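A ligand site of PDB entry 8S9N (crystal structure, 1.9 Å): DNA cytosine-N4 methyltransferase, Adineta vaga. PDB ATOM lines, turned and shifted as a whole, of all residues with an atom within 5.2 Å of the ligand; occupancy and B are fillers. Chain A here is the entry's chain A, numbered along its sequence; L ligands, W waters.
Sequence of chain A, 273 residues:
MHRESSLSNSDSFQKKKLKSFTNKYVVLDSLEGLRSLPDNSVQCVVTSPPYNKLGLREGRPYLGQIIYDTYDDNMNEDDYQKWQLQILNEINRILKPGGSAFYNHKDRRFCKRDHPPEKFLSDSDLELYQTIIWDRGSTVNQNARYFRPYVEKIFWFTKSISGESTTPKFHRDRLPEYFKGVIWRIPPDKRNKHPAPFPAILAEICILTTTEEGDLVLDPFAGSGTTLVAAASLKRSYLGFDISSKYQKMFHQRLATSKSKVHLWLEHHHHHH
Water W3 lies within hydrogen-bond range of N1 of the ligand (2.4 Å), O of Phe 221 (2.6 Å), OD2 of Asp 219 (2.8 Å), N of Ser 48 (3.0 Å) and OG1 of Thr 47 (3.4 Å).
Water W4 lies within hydrogen-bond range of the side-chain hydroxyl (OG) of Ser 48 (2.7 Å), a nitrogen (N2) of the ligand (2.7 Å) and the backbone carbonyl oxygen (O) of Pro 49 (3.1 Å).
Water W1 lies within hydrogen-bond range of the backbone carbonyl oxygen of Ala 196 (2.6 Å), a nitrogen (N1) of the ligand (3.3 Å) and the backbone NH of Phe 198 (3.4 Å).
The backbone NH (N) of Ser 224 lies within hydrogen-bond range of an oxygen (O2) of the ligand.
The side-chain hydroxyl of Ser 224 sits at hydrogen-bond distance from an oxygen (O2) of the ligand (2.7 Å).
O5 of the ligand lies within hydrogen-bond range of OD1 of Asp 242.
N of Ser 30 sits at hydrogen-bond distance from N6 of the ligand, at 3.0 Å.
O4 of the ligand is in hydrogen-bond range of NE2 of His 194 (3.0 Å).
OG1 of Thr 226 is in hydrogen-bond range of O1 of the ligand (3.1 Å).
N2 of the ligand sits at hydrogen-bond distance from O of Ala 196, 3.2 Å away.
An oxygen (O1) of the ligand is in hydrogen-bond range of the backbone NH (N) of Phe 198 (3.3 Å).
N5 of the ligand sits at hydrogen-bond distance from OD1 of Asp 29 (3.3 Å).
N1 of the ligand is in salt-bridge range of OD2 of Asp 219 (3.96 Å).
The side-chain amide nitrogen (ND2) of Asn 192 lies within hydrogen-bond range of the side-chain hydroxyl (OG) of Ser 224 (3.4 Å).
The backbone NH (N) of Leu 28 is in hydrogen-bond range of the backbone carbonyl oxygen (O) of Asp 242, at 2.7 Å.
N of His 194 lies within hydrogen-bond range of OD1 of Asn 192, at 2.8 Å.
N of Phe 221 sits at hydrogen-bond distance from O of Phe 241.
The backbone carbonyl oxygen of Phe 241 sits at hydrogen-bond distance from the backbone NH of Ala 222, at 3.0 Å.
The backbone carbonyl oxygen of Asp 219 sits at hydrogen-bond distance from the backbone NH of Phe 241 (3.0 Å).
The side-chain carboxylate of Asp 219 sits at hydrogen-bond distance from the side-chain hydroxyl of Thr 47 (2.7 Å).
OD2 of Asp 219 sits at hydrogen-bond distance from OG1 of Thr 227, at 2.9 Å.
Residues that only touch the ligand: Tyr 247 (3.1 Å), Phe 221 (3.2 Å), Pro 50 (3.3 Å), Gly 223 (3.3 Å), Pro 197 (3.3 Å), Ala 222 (3.5 Å), Ser 48 (3.6 Å), Tyr 51 (3.6 Å), Ile 243 (3.6 Å), Trp 83 (3.7 Å), Pro 220 (3.9 Å) and Leu 28 (3.96 Å).
Hydrophobic or aromatic side chains within 4 Å of the ligand: Pro 50, Tyr 51, Trp 83, His 194, Pro 197, Phe 198, Phe 221, Ile 243 and Tyr 247.
Within 4 Å of the ligand: Leu 28, Asp 29, Ser 30, Ser 48, Pro 50, Tyr 51, Trp 83, His 194, Ala 196, Pro 197, Phe 198, Asp 219, Pro 220, Phe 221, Ala 222, Gly 223, Ser 224, Thr 226, Asp 242, Ile 243 and Tyr 247.
Along chain A the residues within 4 Å of the ligand span positions 28 to 247.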
ATOM      1  N   LEU A  28     -28.408 -14.275  29.519  1.00  0.00           N
ATOM      2  CA  LEU A  28     -29.299 -15.419  29.655  1.00  0.00           C
ATOM      3  C   LEU A  28     -28.781 -16.538  28.774  1.00  0.00           C
ATOM      4  O   LEU A  28     -28.186 -16.291  27.721  1.00  0.00           O
ATOM      5  CB  LEU A  28     -30.732 -15.046  29.267  1.00  0.00           C
ATOM      6  CG  LEU A  28     -31.848 -15.995  29.686  1.00  0.00           C
ATOM      7  CD1 LEU A  28     -31.846 -16.155  31.188  1.00  0.00           C
ATOM      8  CD2 LEU A  28     -33.178 -15.454  29.198  1.00  0.00           C
ATOM      9  N   ASP A  29     -29.028 -17.777  29.206  1.00  0.00           N
ATOM     10  CA  ASP A  29     -28.737 -18.929  28.375  1.00  0.00           C
ATOM     11  C   ASP A  29     -29.487 -18.817  27.049  1.00  0.00           C
ATOM     12  O   ASP A  29     -30.661 -18.425  27.017  1.00  0.00           O
ATOM     13  CB  ASP A  29     -29.114 -20.227  29.089  1.00  0.00           C
ATOM     14  CG  ASP A  29     -29.020 -21.441  28.188  1.00  0.00           C
ATOM     15  OD1 ASP A  29     -27.935 -21.690  27.629  1.00  0.00           O
ATOM     16  OD2 ASP A  29     -30.049 -22.138  28.031  1.00  0.00           O
ATOM     17  N   SER A  30     -28.795 -19.150  25.952  1.00  0.00           N
ATOM     18  CA  SER A  30     -29.351 -18.927  24.619  1.00  0.00           C
ATOM     19  C   SER A  30     -30.658 -19.687  24.421  1.00  0.00           C
ATOM     20  O   SER A  30     -31.658 -19.107  23.988  1.00  0.00           O
ATOM     21  CB  SER A  30     -28.332 -19.340  23.561  1.00  0.00           C
ATOM     22  OG  SER A  30     -28.854 -19.171  22.257  1.00  0.00           O
ATOM     23  N   THR A  47     -26.307 -14.593  13.605  1.00  0.00           N
ATOM     24  CA  THR A  47     -25.602 -15.123  14.751  1.00  0.00           C
ATOM     25  C   THR A  47     -24.455 -16.017  14.305  1.00  0.00           C
ATOM     26  O   THR A  47     -24.482 -16.594  13.208  1.00  0.00           O
ATOM     27  CB  THR A  47     -26.545 -15.904  15.674  1.00  0.00           C
ATOM     28  OG1 THR A  47     -25.877 -16.207  16.901  1.00  0.00           O
ATOM     29  CG2 THR A  47     -27.009 -17.194  15.008  1.00  0.00           C
ATOM     30  N   SER A  48     -23.449 -16.134  15.166  1.00  0.00           N
ATOM     31  CA  SER A  48     -22.351 -17.086  14.973  1.00  0.00           C
ATOM     32  C   SER A  48     -22.208 -17.871  16.272  1.00  0.00           C
ATOM     33  O   SER A  48     -21.858 -17.284  17.310  1.00  0.00           O
ATOM     34  CB  SER A  48     -21.057 -16.369  14.597  1.00  0.00           C
ATOM     35  OG  SER A  48     -20.004 -17.304  14.388  1.00  0.00           O
ATOM     36  N   PRO A  49     -22.489 -19.172  16.268  1.00  0.00           N
ATOM     37  CA  PRO A  49     -22.550 -19.936  17.525  1.00  0.00           C
ATOM     38  C   PRO A  49     -21.169 -20.200  18.097  1.00  0.00           C
ATOM     39  O   PRO A  49     -20.168 -20.210  17.368  1.00  0.00           O
ATOM     40  CB  PRO A  49     -23.249 -21.234  17.102  1.00  0.00           C
ATOM     41  CG  PRO A  49     -22.869 -21.392  15.676  1.00  0.00           C
ATOM     42  CD  PRO A  49     -22.852 -20.002  15.108  1.00  0.00           C
ATOM     43  N   PRO A  50     -21.096 -20.429  19.420  1.00  0.00           N
ATOM     44  CA  PRO A  50     -19.820 -20.691  20.100  1.00  0.00           C
ATOM     45  C   PRO A  50     -19.365 -22.137  20.118  1.00  0.00           C
ATOM     46  O   PRO A  50     -19.900 -23.003  19.415  1.00  0.00           O
ATOM     47  CB  PRO A  50     -20.105 -20.212  21.521  1.00  0.00           C
ATOM     48  CG  PRO A  50     -21.536 -20.610  21.700  1.00  0.00           C
ATOM     49  CD  PRO A  50     -22.204 -20.353  20.381  1.00  0.00           C
ATOM     50  N   TYR A  51     -18.340 -22.400  20.934  1.00  0.00           N
ATOM     51  CA  TYR A  51     -17.751 -23.723  21.199  1.00  0.00           C
ATOM     52  C   TYR A  51     -17.118 -24.308  19.938  1.00  0.00           C
ATOM     53  O   TYR A  51     -17.385 -25.452  19.585  1.00  0.00           O
ATOM     54  CB  TYR A  51     -18.794 -24.721  21.754  1.00  0.00           C
ATOM     55  CG  TYR A  51     -19.468 -24.331  23.056  1.00  0.00           C
ATOM     56  CD1 TYR A  51     -18.967 -23.344  23.886  1.00  0.00           C
ATOM     57  CD2 TYR A  51     -20.638 -24.980  23.459  1.00  0.00           C
ATOM     58  CE1 TYR A  51     -19.604 -22.994  25.076  1.00  0.00           C
ATOM     59  CE2 TYR A  51     -21.280 -24.649  24.634  1.00  0.00           C
ATOM     60  CZ  TYR A  51     -20.759 -23.658  25.441  1.00  0.00           C
ATOM     61  OH  TYR A  51     -21.410 -23.336  26.611  1.00  0.00           O
ATOM     62  N   TRP A  83     -27.383 -29.947  20.624  1.00  0.00           N
ATOM     63  CA  TRP A  83     -27.679 -28.628  21.181  1.00  0.00           C
ATOM     64  C   TRP A  83     -28.005 -27.624  20.084  1.00  0.00           C
ATOM     65  O   TRP A  83     -28.990 -26.881  20.188  1.00  0.00           O
ATOM     66  CB  TRP A  83     -26.487 -28.155  22.024  1.00  0.00           C
ATOM     67  CG  TRP A  83     -26.569 -26.730  22.485  1.00  0.00           C
ATOM     68  CD1 TRP A  83     -27.602 -26.137  23.135  1.00  0.00           C
ATOM     69  CD2 TRP A  83     -25.553 -25.731  22.353  1.00  0.00           C
ATOM     70  NE1 TRP A  83     -27.313 -24.821  23.404  1.00  0.00           N
ATOM     71  CE2 TRP A  83     -26.054 -24.545  22.938  1.00  0.00           C
ATOM     72  CE3 TRP A  83     -24.258 -25.718  21.803  1.00  0.00           C
ATOM     73  CZ2 TRP A  83     -25.310 -23.364  22.980  1.00  0.00           C
ATOM     74  CZ3 TRP A  83     -23.531 -24.542  21.843  1.00  0.00           C
ATOM     75  CH2 TRP A  83     -24.067 -23.386  22.429  1.00  0.00           C
ATOM     76  N   ASN A 192     -11.846  -5.273  16.795  1.00  0.00           N
ATOM     77  CA  ASN A 192     -12.787  -5.729  17.815  1.00  0.00           C
ATOM     78  C   ASN A 192     -12.066  -6.558  18.860  1.00  0.00           C
ATOM     79  O   ASN A 192     -11.328  -7.485  18.533  1.00  0.00           O
ATOM     80  CB  ASN A 192     -13.915  -6.532  17.163  1.00  0.00           C
ATOM     81  CG  ASN A 192     -15.117  -6.703  18.077  1.00  0.00           C
ATOM     82  OD1 ASN A 192     -14.981  -7.057  19.249  1.00  0.00           O
ATOM     83  ND2 ASN A 192     -16.309  -6.427  17.546  1.00  0.00           N
ATOM     84  N   HIS A 194     -13.427  -8.567  21.036  1.00  0.00           N
ATOM     85  CA  HIS A 194     -14.004  -9.884  21.261  1.00  0.00           C
ATOM     86  C   HIS A 194     -13.124 -10.938  20.596  1.00  0.00           C
ATOM     87  O   HIS A 194     -12.575 -10.706  19.512  1.00  0.00           O
ATOM     88  CB  HIS A 194     -15.423  -9.951  20.691  1.00  0.00           C
ATOM     89  CG  HIS A 194     -16.162 -11.203  21.061  1.00  0.00           C
ATOM     90  ND1 HIS A 194     -16.046 -12.363  20.341  1.00  0.00           N
ATOM     91  CD2 HIS A 194     -17.008 -11.462  22.081  1.00  0.00           C
ATOM     92  CE1 HIS A 194     -16.799 -13.299  20.898  1.00  0.00           C
ATOM     93  NE2 HIS A 194     -17.394 -12.779  21.951  1.00  0.00           N
ATOM     94  N   ALA A 196     -13.793 -13.556  18.963  1.00  0.00           N
ATOM     95  CA  ALA A 196     -14.288 -14.127  17.720  1.00  0.00           C
ATOM     96  C   ALA A 196     -15.582 -13.480  17.258  1.00  0.00           C
ATOM     97  O   ALA A 196     -16.645 -14.117  17.333  1.00  0.00           O
ATOM     98  CB  ALA A 196     -14.486 -15.638  17.892  1.00  0.00           C
ATOM     99  N   PRO A 197     -15.560 -12.217  16.795  1.00  0.00           N
ATOM    100  CA  PRO A 197     -16.773 -11.616  16.213  1.00  0.00           C
ATOM    101  C   PRO A 197     -16.806 -11.698  14.690  1.00  0.00           C
ATOM    102  O   PRO A 197     -15.837 -12.149  14.074  1.00  0.00           O
ATOM    103  CB  PRO A 197     -16.672 -10.160  16.692  1.00  0.00           C
ATOM    104  CG  PRO A 197     -15.200  -9.900  16.636  1.00  0.00           C
ATOM    105  CD  PRO A 197     -14.498 -11.210  16.980  1.00  0.00           C
ATOM    106  N   PHE A 198     -17.916 -11.279  14.087  1.00  0.00           N
ATOM    107  CA  PHE A 198     -17.970 -10.931  12.671  1.00  0.00           C
ATOM    108  C   PHE A 198     -18.189  -9.421  12.523  1.00  0.00           C
ATOM    109  O   PHE A 198     -18.658  -8.767  13.461  1.00  0.00           O
ATOM    110  CB  PHE A 198     -19.061 -11.701  11.903  1.00  0.00           C
ATOM    111  CG  PHE A 198     -20.427 -11.698  12.552  1.00  0.00           C
ATOM    112  CD1 PHE A 198     -21.112 -10.514  12.774  1.00  0.00           C
ATOM    113  CD2 PHE A 198     -21.031 -12.889  12.922  1.00  0.00           C
ATOM    114  CE1 PHE A 198     -22.361 -10.519  13.367  1.00  0.00           C
ATOM    115  CE2 PHE A 198     -22.276 -12.902  13.504  1.00  0.00           C
ATOM    116  CZ  PHE A 198     -22.945 -11.713  13.728  1.00  0.00           C
ATOM    117  N   ASP A 219     -30.012 -11.843  17.989  1.00  0.00           N
ATOM    118  CA  ASP A 219     -28.773 -12.618  17.984  1.00  0.00           C
ATOM    119  C   ASP A 219     -28.707 -13.390  19.294  1.00  0.00           C
ATOM    120  O   ASP A 219     -28.451 -12.800  20.355  1.00  0.00           O
ATOM    121  CB  ASP A 219     -27.528 -11.744  17.812  1.00  0.00           C
ATOM    122  CG  ASP A 219     -26.246 -12.566  17.614  1.00  0.00           C
ATOM    123  OD1 ASP A 219     -26.224 -13.757  17.971  1.00  0.00           O
ATOM    124  OD2 ASP A 219     -25.253 -12.025  17.072  1.00  0.00           O
ATOM    125  N   PRO A 220     -28.935 -14.696  19.265  1.00  0.00           N
ATOM    126  CA  PRO A 220     -28.930 -15.498  20.499  1.00  0.00           C
ATOM    127  C   PRO A 220     -27.543 -15.799  21.053  1.00  0.00           C
ATOM    128  O   PRO A 220     -27.441 -16.468  22.085  1.00  0.00           O
ATOM    129  CB  PRO A 220     -29.652 -16.773  20.070  1.00  0.00           C
ATOM    130  CG  PRO A 220     -29.344 -16.902  18.594  1.00  0.00           C
ATOM    131  CD  PRO A 220     -29.277 -15.496  18.066  1.00  0.00           C
ATOM    132  N   PHE A 221     -26.474 -15.326  20.387  1.00  0.00           N
ATOM    133  CA  PHE A 221     -25.072 -15.443  20.848  1.00  0.00           C
ATOM    134  C   PHE A 221     -24.381 -14.089  20.649  1.00  0.00           C
ATOM    135  O   PHE A 221     -23.442 -13.951  19.871  1.00  0.00           O
ATOM    136  CB  PHE A 221     -24.328 -16.577  20.143  1.00  0.00           C
ATOM    137  CG  PHE A 221     -24.961 -17.924  20.345  1.00  0.00           C
ATOM    138  CD1 PHE A 221     -24.853 -18.595  21.556  1.00  0.00           C
ATOM    139  CD2 PHE A 221     -25.651 -18.525  19.319  1.00  0.00           C
ATOM    140  CE1 PHE A 221     -25.439 -19.847  21.725  1.00  0.00           C
ATOM    141  CE2 PHE A 221     -26.237 -19.771  19.476  1.00  0.00           C
ATOM    142  CZ  PHE A 221     -26.128 -20.421  20.681  1.00  0.00           C
ATOM    143  N   ALA A 222     -24.936 -13.049  21.282  1.00  0.00           N
ATOM    144  CA  ALA A 222     -24.672 -11.673  20.868  1.00  0.00           C
ATOM    145  C   ALA A 222     -23.205 -11.283  21.013  1.00  0.00           C
ATOM    146  O   ALA A 222     -22.707 -10.443  20.251  1.00  0.00           O
ATOM    147  CB  ALA A 222     -25.578 -10.722  21.649  1.00  0.00           C
ATOM    148  N   GLY A 223     -22.499 -11.829  22.004  1.00  0.00           N
ATOM    149  CA  GLY A 223     -21.088 -11.486  22.164  1.00  0.00           C
ATOM    150  C   GLY A 223     -20.906  -9.984  22.354  1.00  0.00           C
ATOM    151  O   GLY A 223     -21.554  -9.360  23.205  1.00  0.00           O
ATOM    152  N   SER A 224     -20.040  -9.386  21.532  1.00  0.00           N
ATOM    153  CA  SER A 224     -19.803  -7.949  21.607  1.00  0.00           C
ATOM    154  C   SER A 224     -21.003  -7.117  21.172  1.00  0.00           C
ATOM    155  O   SER A 224     -20.991  -5.902  21.373  1.00  0.00           O
ATOM    156  CB  SER A 224     -18.586  -7.563  20.762  1.00  0.00           C
ATOM    157  OG  SER A 224     -18.801  -7.818  19.390  1.00  0.00           O
ATOM    158  N   GLY A 225     -22.028  -7.736  20.576  1.00  0.00           N
ATOM    159  CA  GLY A 225     -23.226  -7.008  20.185  1.00  0.00           C
ATOM    160  C   GLY A 225     -23.223  -6.479  18.770  1.00  0.00           C
ATOM    161  O   GLY A 225     -24.047  -5.611  18.459  1.00  0.00           O
ATOM    162  N   THR A 226     -22.342  -6.977  17.912  1.00  0.00           N
ATOM    163  CA  THR A 226     -22.247  -6.495  16.531  1.00  0.00           C
ATOM    164  C   THR A 226     -23.595  -6.509  15.822  1.00  0.00           C
ATOM    165  O   THR A 226     -23.956  -5.552  15.116  1.00  0.00           O
ATOM    166  CB  THR A 226     -21.254  -7.360  15.745  1.00  0.00           C
ATOM    167  OG1 THR A 226     -19.979  -7.340  16.409  1.00  0.00           O
ATOM    168  CG2 THR A 226     -21.098  -6.823  14.344  1.00  0.00           C
ATOM    169  N   THR A 227     -24.351  -7.599  15.971  1.00  0.00           N
ATOM    170  CA  THR A 227     -25.665  -7.669  15.338  1.00  0.00           C
ATOM    171  C   THR A 227     -26.599  -6.591  15.865  1.00  0.00           C
ATOM    172  O   THR A 227     -27.351  -5.981  15.100  1.00  0.00           O
ATOM    173  CB  THR A 227     -26.272  -9.059  15.560  1.00  0.00           C
ATOM    174  OG1 THR A 227     -25.423 -10.053  14.977  1.00  0.00           O
ATOM    175  CG2 THR A 227     -27.664  -9.138  14.945  1.00  0.00           C
ATOM    176  N   PHE A 241     -29.072 -12.362  23.235  1.00  0.00           N
ATOM    177  CA  PHE A 241     -28.851 -13.233  24.377  1.00  0.00           C
ATOM    178  C   PHE A 241     -27.394 -13.614  24.427  1.00  0.00           C
ATOM    179  O   PHE A 241     -26.794 -13.933  23.406  1.00  0.00           O
ATOM    180  CB  PHE A 241     -29.695 -14.505  24.315  1.00  0.00           C
ATOM    181  CG  PHE A 241     -31.161 -14.268  24.291  1.00  0.00           C
ATOM    182  CD1 PHE A 241     -31.794 -13.647  25.352  1.00  0.00           C
ATOM    183  CD2 PHE A 241     -31.919 -14.693  23.213  1.00  0.00           C
ATOM    184  CE1 PHE A 241     -33.159 -13.431  25.328  1.00  0.00           C
ATOM    185  CE2 PHE A 241     -33.281 -14.491  23.191  1.00  0.00           C
ATOM    186  CZ  PHE A 241     -33.905 -13.853  24.243  1.00  0.00           C
ATOM    187  N   ASP A 242     -26.818 -13.556  25.619  1.00  0.00           N
ATOM    188  CA  ASP A 242     -25.483 -14.088  25.830  1.00  0.00           C
ATOM    189  C   ASP A 242     -25.339 -14.378  27.313  1.00  0.00           C
ATOM    190  O   ASP A 242     -26.110 -13.873  28.137  1.00  0.00           O
ATOM    191  CB  ASP A 242     -24.401 -13.134  25.335  1.00  0.00           C
ATOM    192  CG  ASP A 242     -23.043 -13.814  25.204  1.00  0.00           C
ATOM    193  OD1 ASP A 242     -22.608 -14.486  26.162  1.00  0.00           O
ATOM    194  OD2 ASP A 242     -22.431 -13.674  24.132  1.00  0.00           O
ATOM    195  N   ILE A 243     -24.349 -15.211  27.659  1.00  0.00           N
ATOM    196  CA  ILE A 243     -24.125 -15.513  29.059  1.00  0.00           C
ATOM    197  C   ILE A 243     -23.027 -14.669  29.683  1.00  0.00           C
ATOM    198  O   ILE A 243     -22.706 -14.877  30.856  1.00  0.00           O
ATOM    199  CB  ILE A 243     -23.709 -16.977  29.272  1.00  0.00           C
ATOM    200  CG1 ILE A 243     -22.594 -17.309  28.285  1.00  0.00           C
ATOM    201  CG2 ILE A 243     -24.899 -17.891  29.152  1.00  0.00           C
ATOM    202  CD1 ILE A 243     -21.913 -18.595  28.554  1.00  0.00           C
ATOM    203  N   SER A 244     -22.390 -13.766  28.929  1.00  0.00           N
ATOM    204  CA  SER A 244     -21.307 -12.958  29.467  1.00  0.00           C
ATOM    205  C   SER A 244     -21.873 -11.602  29.864  1.00  0.00           C
ATOM    206  O   SER A 244     -22.275 -10.803  28.997  1.00  0.00           O
ATOM    207  CB  SER A 244     -20.161 -12.748  28.491  1.00  0.00           C
ATOM    208  OG  SER A 244     -19.110 -12.066  29.140  1.00  0.00           O
ATOM    209  N   TYR A 247     -19.601  -9.283  28.239  1.00  0.00           N
ATOM    210  CA  TYR A 247     -19.927  -8.861  26.885  1.00  0.00           C
ATOM    211  C   TYR A 247     -21.122  -7.911  26.864  1.00  0.00           C
ATOM    212  O   TYR A 247     -21.182  -7.022  26.014  1.00  0.00           O
ATOM    213  CB  TYR A 247     -20.166 -10.094  25.993  1.00  0.00           C
ATOM    214  CG  TYR A 247     -18.923 -10.948  25.786  1.00  0.00           C
ATOM    215  CD1 TYR A 247     -17.655 -10.428  26.012  1.00  0.00           C
ATOM    216  CD2 TYR A 247     -19.013 -12.268  25.386  1.00  0.00           C
ATOM    217  CE1 TYR A 247     -16.511 -11.185  25.833  1.00  0.00           C
ATOM    218  CE2 TYR A 247     -17.876 -13.049  25.204  1.00  0.00           C
ATOM    219  CZ  TYR A 247     -16.634 -12.498  25.436  1.00  0.00           C
ATOM    220  OH  TYR A 247     -15.495 -13.264  25.261  1.00  0.00           O
HETATM  221  N1  LIG L   1     -21.369 -12.699  16.752  1.00  0.00           N
HETATM  222  C1  LIG L   1     -20.718 -12.183  17.965  1.00  0.00           C
HETATM  223  C2  LIG L   1     -20.038 -10.850  17.663  1.00  0.00           C
HETATM  224  O1  LIG L   1     -19.983 -10.395  16.534  1.00  0.00           O
HETATM  225  O2  LIG L   1     -19.529 -10.282  18.718  1.00  0.00           O
HETATM  226  C3  LIG L   1     -19.732 -13.196  18.546  1.00  0.00           C
HETATM  227  C4  LIG L   1     -20.419 -14.491  19.014  1.00  0.00           C
HETATM  228  C5  LIG L   1     -19.488 -15.527  19.639  1.00  0.00           C
HETATM  229  N2  LIG L   1     -18.664 -16.181  18.605  1.00  0.00           N
HETATM  230  C6  LIG L   1     -20.230 -16.595  20.446  1.00  0.00           C
HETATM  231  C7  LIG L   1     -20.789 -16.096  21.771  1.00  0.00           C
HETATM  232  O3  LIG L   1     -21.667 -17.073  22.353  1.00  0.00           O
HETATM  233  C8  LIG L   1     -19.739 -15.756  22.837  1.00  0.00           C
HETATM  234  O4  LIG L   1     -19.714 -14.346  23.068  1.00  0.00           O
HETATM  235  C9  LIG L   1     -20.187 -16.548  24.075  1.00  0.00           C
HETATM  236  O5  LIG L   1     -20.116 -15.762  25.264  1.00  0.00           O
HETATM  237  C10 LIG L   1     -21.648 -16.868  23.753  1.00  0.00           C
HETATM  238  N3  LIG L   1     -22.182 -18.057  24.406  1.00  0.00           N
HETATM  239  C11 LIG L   1     -21.522 -19.231  24.672  1.00  0.00           C
HETATM  240  N4  LIG L   1     -22.281 -20.176  25.154  1.00  0.00           N
HETATM  241  C12 LIG L   1     -23.535 -19.588  25.220  1.00  0.00           C
HETATM  242  C13 LIG L   1     -24.787 -20.064  25.648  1.00  0.00           C
HETATM  243  N5  LIG L   1     -25.019 -21.318  26.041  1.00  0.00           N
HETATM  244  N6  LIG L   1     -25.828 -19.202  25.627  1.00  0.00           N
HETATM  245  C14 LIG L   1     -25.626 -17.951  25.193  1.00  0.00           C
HETATM  246  N7  LIG L   1     -24.488 -17.395  24.746  1.00  0.00           N
HETATM  247  C15 LIG L   1     -23.476 -18.270  24.784  1.00  0.00           C
HETATM  248  O   HOH W   1     -18.602 -14.231  15.662  1.00  0.00           O
HETATM  249  O   HOH W   2     -16.494 -17.044  21.127  1.00  0.00           O
HETATM  250  O   HOH W   3     -23.354 -14.021  17.240  1.00  0.00           O
HETATM  251  O   HOH W   4     -18.457 -17.803  16.500  1.00  0.00           O
